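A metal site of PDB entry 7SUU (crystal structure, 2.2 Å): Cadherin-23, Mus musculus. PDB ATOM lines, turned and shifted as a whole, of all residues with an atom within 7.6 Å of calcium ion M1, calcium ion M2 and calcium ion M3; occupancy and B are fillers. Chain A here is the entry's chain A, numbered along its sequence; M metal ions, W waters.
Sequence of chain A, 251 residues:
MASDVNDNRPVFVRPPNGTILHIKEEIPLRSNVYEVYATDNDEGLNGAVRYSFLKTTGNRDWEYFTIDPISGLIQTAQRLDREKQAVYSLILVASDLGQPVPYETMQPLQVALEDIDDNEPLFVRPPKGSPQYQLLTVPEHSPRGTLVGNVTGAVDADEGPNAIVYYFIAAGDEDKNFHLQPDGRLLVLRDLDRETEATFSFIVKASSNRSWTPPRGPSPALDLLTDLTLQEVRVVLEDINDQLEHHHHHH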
ATOM      1  N   GLU A  25      19.854  -0.683  28.914  1.00  0.00           N
ATOM      2  CA  GLU A  25      19.976  -0.145  27.546  1.00  0.00           C
ATOM      3  C   GLU A  25      19.106  -1.007  26.592  1.00  0.00           C
ATOM      4  O   GLU A  25      18.690  -2.123  26.986  1.00  0.00           O
ATOM      5  CB  GLU A  25      21.453  -0.092  27.131  1.00  0.00           C
ATOM      6  CG  GLU A  25      22.067  -1.452  26.923  1.00  0.00           C
ATOM      7  CD  GLU A  25      23.339  -1.480  26.110  1.00  0.00           C
ATOM      8  OE1 GLU A  25      24.185  -2.269  26.470  1.00  0.00           O
ATOM      9  OE2 GLU A  25      23.450  -0.737  25.102  1.00  0.00           O
ATOM     10  N   GLU A  26      18.825  -0.487  25.398  1.00  0.00           N
ATOM     11  CA  GLU A  26      18.174  -1.189  24.255  1.00  0.00           C
ATOM     12  C   GLU A  26      16.735  -1.624  24.594  1.00  0.00           C
ATOM     13  O   GLU A  26      16.176  -2.454  23.857  1.00  0.00           O
ATOM     14  CB  GLU A  26      19.017  -2.397  23.808  1.00  0.00           C
ATOM     15  CG  GLU A  26      20.455  -2.045  23.405  1.00  0.00           C
ATOM     16  CD  GLU A  26      20.678  -1.093  22.239  1.00  0.00           C
ATOM     17  OE1 GLU A  26      19.691  -0.635  21.626  1.00  0.00           O
ATOM     18  OE2 GLU A  26      21.870  -0.796  21.932  1.00  0.00           O
ATOM     19  N   ARG A  79      15.941   4.954  20.433  1.00  0.00           N
ATOM     20  CA  ARG A  79      16.845   3.871  20.830  1.00  0.00           C
ATOM     21  C   ARG A  79      17.745   4.413  21.935  1.00  0.00           C
ATOM     22  O   ARG A  79      18.236   5.538  21.784  1.00  0.00           O
ATOM     23  CB  ARG A  79      17.730   3.434  19.663  1.00  0.00           C
ATOM     24  CG  ARG A  79      18.607   2.252  20.038  1.00  0.00           C
ATOM     25  CD  ARG A  79      19.470   1.821  18.877  1.00  0.00           C
ATOM     26  NE  ARG A  79      20.361   0.755  19.309  1.00  0.00           N
ATOM     27  CZ  ARG A  79      21.430   0.355  18.623  1.00  0.00           C
ATOM     28  NH1 ARG A  79      22.174  -0.642  19.092  1.00  0.00           N
ATOM     29  NH2 ARG A  79      21.717   0.921  17.481  1.00  0.00           N
ATOM     30  N   LEU A  80      17.964   3.611  22.984  1.00  0.00           N
ATOM     31  CA  LEU A  80      18.911   3.949  24.076  1.00  0.00           C
ATOM     32  C   LEU A  80      20.061   2.947  24.031  1.00  0.00           C
ATOM     33  O   LEU A  80      19.897   1.849  24.548  1.00  0.00           O
ATOM     34  CB  LEU A  80      18.166   3.926  25.419  1.00  0.00           C
ATOM     35  CG  LEU A  80      17.185   5.080  25.634  1.00  0.00           C
ATOM     36  CD1 LEU A  80      16.323   4.825  26.860  1.00  0.00           C
ATOM     37  CD2 LEU A  80      17.916   6.406  25.783  1.00  0.00           C
ATOM     38  N   ASP A  81      21.198   3.373  23.489  1.00  0.00           N
ATOM     39  CA  ASP A  81      22.403   2.546  23.261  1.00  0.00           C
ATOM     40  C   ASP A  81      23.507   3.051  24.190  1.00  0.00           C
ATOM     41  O   ASP A  81      23.962   4.187  23.974  1.00  0.00           O
ATOM     42  CB  ASP A  81      22.836   2.589  21.785  1.00  0.00           C
ATOM     43  CG  ASP A  81      24.020   1.675  21.486  1.00  0.00           C
ATOM     44  OD1 ASP A  81      24.399   0.877  22.351  1.00  0.00           O
ATOM     45  OD2 ASP A  81      24.566   1.798  20.383  1.00  0.00           O
ATOM     46  N   ARG A  82      23.915   2.230  25.169  1.00  0.00           N
ATOM     47  CA  ARG A  82      24.892   2.635  26.205  1.00  0.00           C
ATOM     48  C   ARG A  82      26.217   2.866  25.494  1.00  0.00           C
ATOM     49  O   ARG A  82      26.942   3.752  25.933  1.00  0.00           O
ATOM     50  CB  ARG A  82      25.029   1.579  27.315  1.00  0.00           C
ATOM     51  CG  ARG A  82      25.990   1.941  28.443  1.00  0.00           C
ATOM     52  CD  ARG A  82      26.590   0.709  29.133  1.00  0.00           C
ATOM     53  NE  ARG A  82      27.521   0.060  28.215  1.00  0.00           N
ATOM     54  CZ  ARG A  82      28.766   0.462  27.989  1.00  0.00           C
ATOM     55  NH1 ARG A  82      29.507  -0.148  27.085  1.00  0.00           N
ATOM     56  NH2 ARG A  82      29.278   1.477  28.674  1.00  0.00           N
ATOM     57  N   GLU A  83      26.472   2.124  24.415  1.00  0.00           N
ATOM     58  CA  GLU A  83      27.709   2.252  23.601  1.00  0.00           C
ATOM     59  C   GLU A  83      27.666   3.547  22.792  1.00  0.00           C
ATOM     60  O   GLU A  83      28.732   3.979  22.339  1.00  0.00           O
ATOM     61  CB  GLU A  83      27.915   1.019  22.711  1.00  0.00           C
ATOM     62  CG  GLU A  83      28.394  -0.208  23.495  1.00  0.00           C
ATOM     63  CD  GLU A  83      27.342  -1.044  24.225  1.00  0.00           C
ATOM     64  OE1 GLU A  83      26.250  -1.286  23.679  1.00  0.00           O
ATOM     65  OE2 GLU A  83      27.617  -1.463  25.347  1.00  0.00           O
ATOM     66  N   LYS A  84      26.496   4.163  22.610  1.00  0.00           N
ATOM     67  CA  LYS A  84      26.404   5.510  21.983  1.00  0.00           C
ATOM     68  C   LYS A  84      26.533   6.575  23.085  1.00  0.00           C
ATOM     69  O   LYS A  84      27.442   7.446  22.993  1.00  0.00           O
ATOM     70  CB  LYS A  84      25.081   5.685  21.244  1.00  0.00           C
ATOM     71  CG  LYS A  84      25.012   6.943  20.384  1.00  0.00           C
ATOM     72  CD  LYS A  84      23.696   7.111  19.666  1.00  0.00           C
ATOM     73  CE  LYS A  84      23.587   8.453  18.974  1.00  0.00           C
ATOM     74  NZ  LYS A  84      22.179   8.913  18.918  1.00  0.00           N
ATOM     75  N   LEU A 113      22.355   4.114  31.758  1.00  0.00           N
ATOM     76  CA  LEU A 113      21.995   2.837  31.100  1.00  0.00           C
ATOM     77  C   LEU A 113      22.896   1.743  31.653  1.00  0.00           C
ATOM     78  O   LEU A 113      24.120   1.896  31.567  1.00  0.00           O
ATOM     79  CB  LEU A 113      22.158   2.962  29.592  1.00  0.00           C
ATOM     80  CG  LEU A 113      21.317   4.036  28.921  1.00  0.00           C
ATOM     81  CD1 LEU A 113      21.485   3.978  27.406  1.00  0.00           C
ATOM     82  CD2 LEU A 113      19.851   3.904  29.329  1.00  0.00           C
ATOM     83  N   GLU A 114      22.306   0.693  32.203  1.00  0.00           N
ATOM     84  CA  GLU A 114      22.983  -0.566  32.585  1.00  0.00           C
ATOM     85  C   GLU A 114      23.329  -1.320  31.276  1.00  0.00           C
ATOM     86  O   GLU A 114      22.508  -1.412  30.372  1.00  0.00           O
ATOM     87  CB  GLU A 114      22.070  -1.296  33.589  1.00  0.00           C
ATOM     88  CG  GLU A 114      22.335  -2.803  33.699  1.00  0.00           C
ATOM     89  CD  GLU A 114      21.480  -3.623  34.670  1.00  0.00           C
ATOM     90  OE1 GLU A 114      21.685  -4.858  34.722  1.00  0.00           O
ATOM     91  OE2 GLU A 114      20.601  -3.036  35.378  1.00  0.00           O
ATOM     92  N   ASP A 115      24.565  -1.790  31.162  1.00  0.00           N
ATOM     93  CA  ASP A 115      25.078  -2.536  29.987  1.00  0.00           C
ATOM     94  C   ASP A 115      24.359  -3.880  29.804  1.00  0.00           C
ATOM     95  O   ASP A 115      24.134  -4.598  30.800  1.00  0.00           O
ATOM     96  CB  ASP A 115      26.572  -2.792  30.168  1.00  0.00           C
ATOM     97  CG  ASP A 115      27.186  -3.393  28.926  1.00  0.00           C
ATOM     98  OD1 ASP A 115      27.037  -2.791  27.787  1.00  0.00           O
ATOM     99  OD2 ASP A 115      27.819  -4.427  29.107  1.00  0.00           O
ATOM    100  N   ILE A 116      24.033  -4.242  28.567  1.00  0.00           N
ATOM    101  CA  ILE A 116      23.691  -5.646  28.207  1.00  0.00           C
ATOM    102  C   ILE A 116      24.728  -6.138  27.187  1.00  0.00           C
ATOM    103  O   ILE A 116      25.382  -5.289  26.526  1.00  0.00           O
ATOM    104  CB  ILE A 116      22.256  -5.780  27.661  1.00  0.00           C
ATOM    105  CG1 ILE A 116      22.149  -5.192  26.255  1.00  0.00           C
ATOM    106  CG2 ILE A 116      21.233  -5.182  28.632  1.00  0.00           C
ATOM    107  CD1 ILE A 116      20.784  -5.394  25.607  1.00  0.00           C
ATOM    108  N   ASP A 117      24.849  -7.455  27.086  1.00  0.00           N
ATOM    109  CA  ASP A 117      25.861  -8.126  26.250  1.00  0.00           C
ATOM    110  C   ASP A 117      25.358  -8.120  24.821  1.00  0.00           C
ATOM    111  O   ASP A 117      24.880  -9.166  24.385  1.00  0.00           O
ATOM    112  CB  ASP A 117      26.155  -9.542  26.736  1.00  0.00           C
ATOM    113  CG  ASP A 117      27.366 -10.187  26.070  1.00  0.00           C
ATOM    114  OD1 ASP A 117      28.070  -9.502  25.249  1.00  0.00           O
ATOM    115  OD2 ASP A 117      27.629 -11.345  26.393  1.00  0.00           O
ATOM    116  N   ASP A 118      25.419  -6.985  24.130  1.00  0.00           N
ATOM    117  CA  ASP A 118      24.850  -6.891  22.755  1.00  0.00           C
ATOM    118  C   ASP A 118      25.956  -6.569  21.759  1.00  0.00           C
ATOM    119  O   ASP A 118      25.618  -6.164  20.655  1.00  0.00           O
ATOM    120  CB  ASP A 118      23.730  -5.833  22.639  1.00  0.00           C
ATOM    121  CG  ASP A 118      24.128  -4.437  23.114  1.00  0.00           C
ATOM    122  OD1 ASP A 118      25.108  -4.321  23.882  1.00  0.00           O
ATOM    123  OD2 ASP A 118      23.449  -3.487  22.733  1.00  0.00           O
ATOM    124  N   ASN A 119      27.223  -6.781  22.121  1.00  0.00           N
ATOM    125  CA  ASN A 119      28.360  -6.605  21.183  1.00  0.00           C
ATOM    126  C   ASN A 119      29.275  -7.812  21.298  1.00  0.00           C
ATOM    127  O   ASN A 119      29.350  -8.400  22.377  1.00  0.00           O
ATOM    128  CB  ASN A 119      29.114  -5.304  21.453  1.00  0.00           C
ATOM    129  CG  ASN A 119      28.259  -4.096  21.121  1.00  0.00           C
ATOM    130  OD1 ASN A 119      27.413  -3.675  21.915  1.00  0.00           O
ATOM    131  ND2 ASN A 119      28.451  -3.551  19.932  1.00  0.00           N
ATOM    132  N   GLU A 120      30.003  -8.119  20.244  1.00  0.00           N
ATOM    133  CA  GLU A 120      30.997  -9.216  20.278  1.00  0.00           C
ATOM    134  C   GLU A 120      32.358  -8.604  19.985  1.00  0.00           C
ATOM    135  O   GLU A 120      32.446  -7.513  19.401  1.00  0.00           O
ATOM    136  CB  GLU A 120      30.648 -10.320  19.288  1.00  0.00           C
ATOM    137  CG  GLU A 120      30.652  -9.861  17.851  1.00  0.00           C
ATOM    138  CD  GLU A 120      30.142 -10.888  16.840  1.00  0.00           C
ATOM    139  OE1 GLU A 120      30.172 -10.585  15.631  1.00  0.00           O
ATOM    140  OE2 GLU A 120      29.736 -11.991  17.263  1.00  0.00           O
ATOM    141  N   PRO A 121      33.461  -9.315  20.369  1.00  0.00           N
ATOM    142  CA  PRO A 121      34.810  -8.921  19.970  1.00  0.00           C
ATOM    143  C   PRO A 121      34.932  -8.775  18.453  1.00  0.00           C
ATOM    144  O   PRO A 121      34.557  -9.687  17.745  1.00  0.00           O
ATOM    145  CB  PRO A 121      35.679 -10.063  20.494  1.00  0.00           C
ATOM    146  CG  PRO A 121      34.916 -10.614  21.638  1.00  0.00           C
ATOM    147  CD  PRO A 121      33.450 -10.508  21.233  1.00  0.00           C
ATOM    148  N   ASP A 156      35.647  -5.611  22.571  1.00  0.00           N
ATOM    149  CA  ASP A 156      34.198  -5.792  22.824  1.00  0.00           C
ATOM    150  C   ASP A 156      33.684  -4.498  23.461  1.00  0.00           C
ATOM    151  O   ASP A 156      34.174  -4.131  24.549  1.00  0.00           O
ATOM    152  CB  ASP A 156      33.964  -7.026  23.693  1.00  0.00           C
ATOM    153  CG  ASP A 156      32.529  -7.482  23.883  1.00  0.00           C
ATOM    154  OD1 ASP A 156      31.669  -6.659  24.209  1.00  0.00           O
ATOM    155  OD2 ASP A 156      32.300  -8.703  23.804  1.00  0.00           O
ATOM    156  N   ALA A 157      32.695  -3.866  22.841  1.00  0.00           N
ATOM    157  CA  ALA A 157      32.212  -2.506  23.203  1.00  0.00           C
ATOM    158  C   ALA A 157      31.373  -2.550  24.486  1.00  0.00           C
ATOM    159  O   ALA A 157      30.993  -1.472  24.980  1.00  0.00           O
ATOM    160  CB  ALA A 157      31.463  -1.876  22.040  1.00  0.00           C
ATOM    161  N   ASP A 158      31.107  -3.743  25.021  1.00  0.00           N
ATOM    162  CA  ASP A 158      30.256  -3.914  26.232  1.00  0.00           C
ATOM    163  C   ASP A 158      31.102  -3.608  27.476  1.00  0.00           C
ATOM    164  O   ASP A 158      32.137  -2.996  27.326  1.00  0.00           O
ATOM    165  CB  ASP A 158      29.595  -5.293  26.249  1.00  0.00           C
ATOM    166  CG  ASP A 158      28.570  -5.505  25.146  1.00  0.00           C
ATOM    167  OD1 ASP A 158      27.873  -4.538  24.764  1.00  0.00           O
ATOM    168  OD2 ASP A 158      28.504  -6.601  24.649  1.00  0.00           O
ATOM    169  N   GLU A 159      30.651  -4.006  28.661  1.00  0.00           N
ATOM    170  CA  GLU A 159      31.255  -3.601  29.966  1.00  0.00           C
ATOM    171  C   GLU A 159      31.593  -4.829  30.822  1.00  0.00           C
ATOM    172  O   GLU A 159      30.794  -5.767  30.897  1.00  0.00           O
ATOM    173  CB  GLU A 159      30.255  -2.713  30.704  1.00  0.00           C
ATOM    174  CG  GLU A 159      30.875  -1.855  31.762  1.00  0.00           C
ATOM    175  CD  GLU A 159      31.477  -0.575  31.233  1.00  0.00           C
ATOM    176  OE1 GLU A 159      32.193  -0.608  30.186  1.00  0.00           O
ATOM    177  OE2 GLU A 159      31.218   0.459  31.859  1.00  0.00           O
ATOM    178  N   GLY A 160      32.750  -4.797  31.477  1.00  0.00           N
ATOM    179  CA  GLY A 160      33.134  -5.807  32.491  1.00  0.00           C
ATOM    180  C   GLY A 160      32.923  -7.214  31.931  1.00  0.00           C
ATOM    181  O   GLY A 160      33.445  -7.536  30.862  1.00  0.00           O
ATOM    182  N   PRO A 161      32.142  -8.081  32.615  1.00  0.00           N
ATOM    183  CA  PRO A 161      32.033  -9.483  32.208  1.00  0.00           C
ATOM    184  C   PRO A 161      31.290  -9.715  30.883  1.00  0.00           C
ATOM    185  O   PRO A 161      31.256 -10.835  30.430  1.00  0.00           O
ATOM    186  CB  PRO A 161      31.339 -10.183  33.391  1.00  0.00           C
ATOM    187  CG  PRO A 161      30.675  -9.054  34.185  1.00  0.00           C
ATOM    188  CD  PRO A 161      31.442  -7.776  33.875  1.00  0.00           C
ATOM    189  N   ASN A 162      30.749  -8.664  30.274  1.00  0.00           N
ATOM    190  CA  ASN A 162      30.109  -8.709  28.939  1.00  0.00           C
ATOM    191  C   ASN A 162      31.149  -8.433  27.848  1.00  0.00           C
ATOM    192  O   ASN A 162      30.798  -8.565  26.667  1.00  0.00           O
ATOM    193  CB  ASN A 162      28.970  -7.696  28.822  1.00  0.00           C
ATOM    194  CG  ASN A 162      27.867  -7.936  29.826  1.00  0.00           C
ATOM    195  OD1 ASN A 162      27.575  -9.076  30.154  1.00  0.00           O
ATOM    196  ND2 ASN A 162      27.249  -6.861  30.303  1.00  0.00           N
ATOM    197  N   ALA A 163      32.387  -8.098  28.216  1.00  0.00           N
ATOM    198  CA  ALA A 163      33.414  -7.598  27.280  1.00  0.00           C
ATOM    199  C   ALA A 163      34.679  -8.460  27.360  1.00  0.00           C
ATOM    200  O   ALA A 163      35.755  -7.932  27.056  1.00  0.00           O
ATOM    201  CB  ALA A 163      33.728  -6.161  27.603  1.00  0.00           C
ATOM    202  N   ILE A 164      34.570  -9.742  27.731  1.00  0.00           N
ATOM    203  CA  ILE A 164      35.770 -10.629  27.794  1.00  0.00           C
ATOM    204  C   ILE A 164      36.198 -10.956  26.374  1.00  0.00           C
ATOM    205  O   ILE A 164      35.355 -11.359  25.598  1.00  0.00           O
ATOM    206  CB  ILE A 164      35.485 -11.885  28.618  1.00  0.00           C
ATOM    207  CG1 ILE A 164      35.150 -11.496  30.062  1.00  0.00           C
ATOM    208  CG2 ILE A 164      36.688 -12.824  28.511  1.00  0.00           C
ATOM    209  CD1 ILE A 164      34.476 -12.573  30.885  1.00  0.00           C
ATOM    210  N   SER A 208      34.165 -14.145  22.877  1.00  0.00           N
ATOM    211  CA  SER A 208      33.887 -14.102  24.330  1.00  0.00           C
ATOM    212  C   SER A 208      33.679 -15.518  24.846  1.00  0.00           C
ATOM    213  O   SER A 208      33.647 -15.688  26.069  1.00  0.00           O
ATOM    214  CB  SER A 208      32.722 -13.183  24.651  1.00  0.00           C
ATOM    215  OG  SER A 208      33.042 -11.833  24.267  1.00  0.00           O
HETATM  216 CA    CA M   1      24.103  -1.286  22.942  1.00  0.00          CA
HETATM  217 CA    CA M   2      26.166  -3.244  25.630  1.00  0.00          CA
HETATM  218 CA    CA M   3      30.034  -8.542  24.584  1.00  0.00          CA
HETATM  219  O   HOH W   1      30.652 -10.885  24.405  1.00  0.00           O
HETATM  220  O   HOH W   2      25.200  -1.879  20.828  1.00  0.00           O
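Along chain A the residues within 4 Å of calcium ion M2 span positions 25 to 158. The nearest printed residue that does not touch calcium ion M2 is Arg 82 (4.4 Å).
Of the 27 residues printed, 5 come within 4 Å of calcium ion M1.
Calcium ion M3 is bound by the backbone carbonyl oxygen (O) of Asn 162 (2.2 Å), the side-chain carboxylate (OD1) of Asp 117 (2.3 Å), the backbone carbonyl oxygen (O) of Asn 119 (2.3 Å), the side-chain carboxylate (OD2) of Asp 156 (2.4 Å), water W1 (2.4 Å), the side-chain carboxylate (OD2) of Asp 158 (2.5 Å) and the side-chain carboxylate (OD1) of Asp 156 (2.5 Å).
OD2 of Asp 115 is in hydrogen-bond range of ND2 of Asn 162 (2.8 Å). OE1 of Glu 83 sits close to OD1 of Asn 119, at 3.2 Å. The guanidinium group (NH1) of Arg 82 sits close to the side-chain carboxylate (OE2) of Glu 83, at 2.9 Å. The side-chain amide oxygen (OD1) of Asn 119 sits close to the side-chain carboxylate (OD1) of Asp 118, 3.1 Å away. OE2 of Glu 25 lies close to N of Arg 82, 3.0 Å away. OD1 of Asp 115 sits close to NE of Arg 82. OG of Ser 208 lies close to OD2 of Asp 156 (3.2 Å). NE of Arg 79 is in salt-bridge range of OE1 of Glu 26 (2.8 Å).
Calcium ion M2 is bound by the side-chain carboxylate (OD1) of Asp 118, the side-chain carboxylate (OD1) of Asp 158, the side-chain carboxylate (OE2) of Glu 83, the side-chain carboxylate (OE1) of Glu 25, the backbone carbonyl oxygen (O) of Ile 116, the side-chain carboxylate (OD1) of Asp 115 and the side-chain carboxylate (OE1) of Glu 83.
Calcium ion M1 is bound by the side-chain carboxylate (OD1) of Asp 81, the side-chain carboxylate (OE1) of Glu 83, the side-chain carboxylate (OD2) of Asp 118, the side-chain carboxylate (OE2) of Glu 25, water W2 and the side-chain carboxylate (OE2) of Glu 26. Calcium ion M1 has six donor atoms within binding distance.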
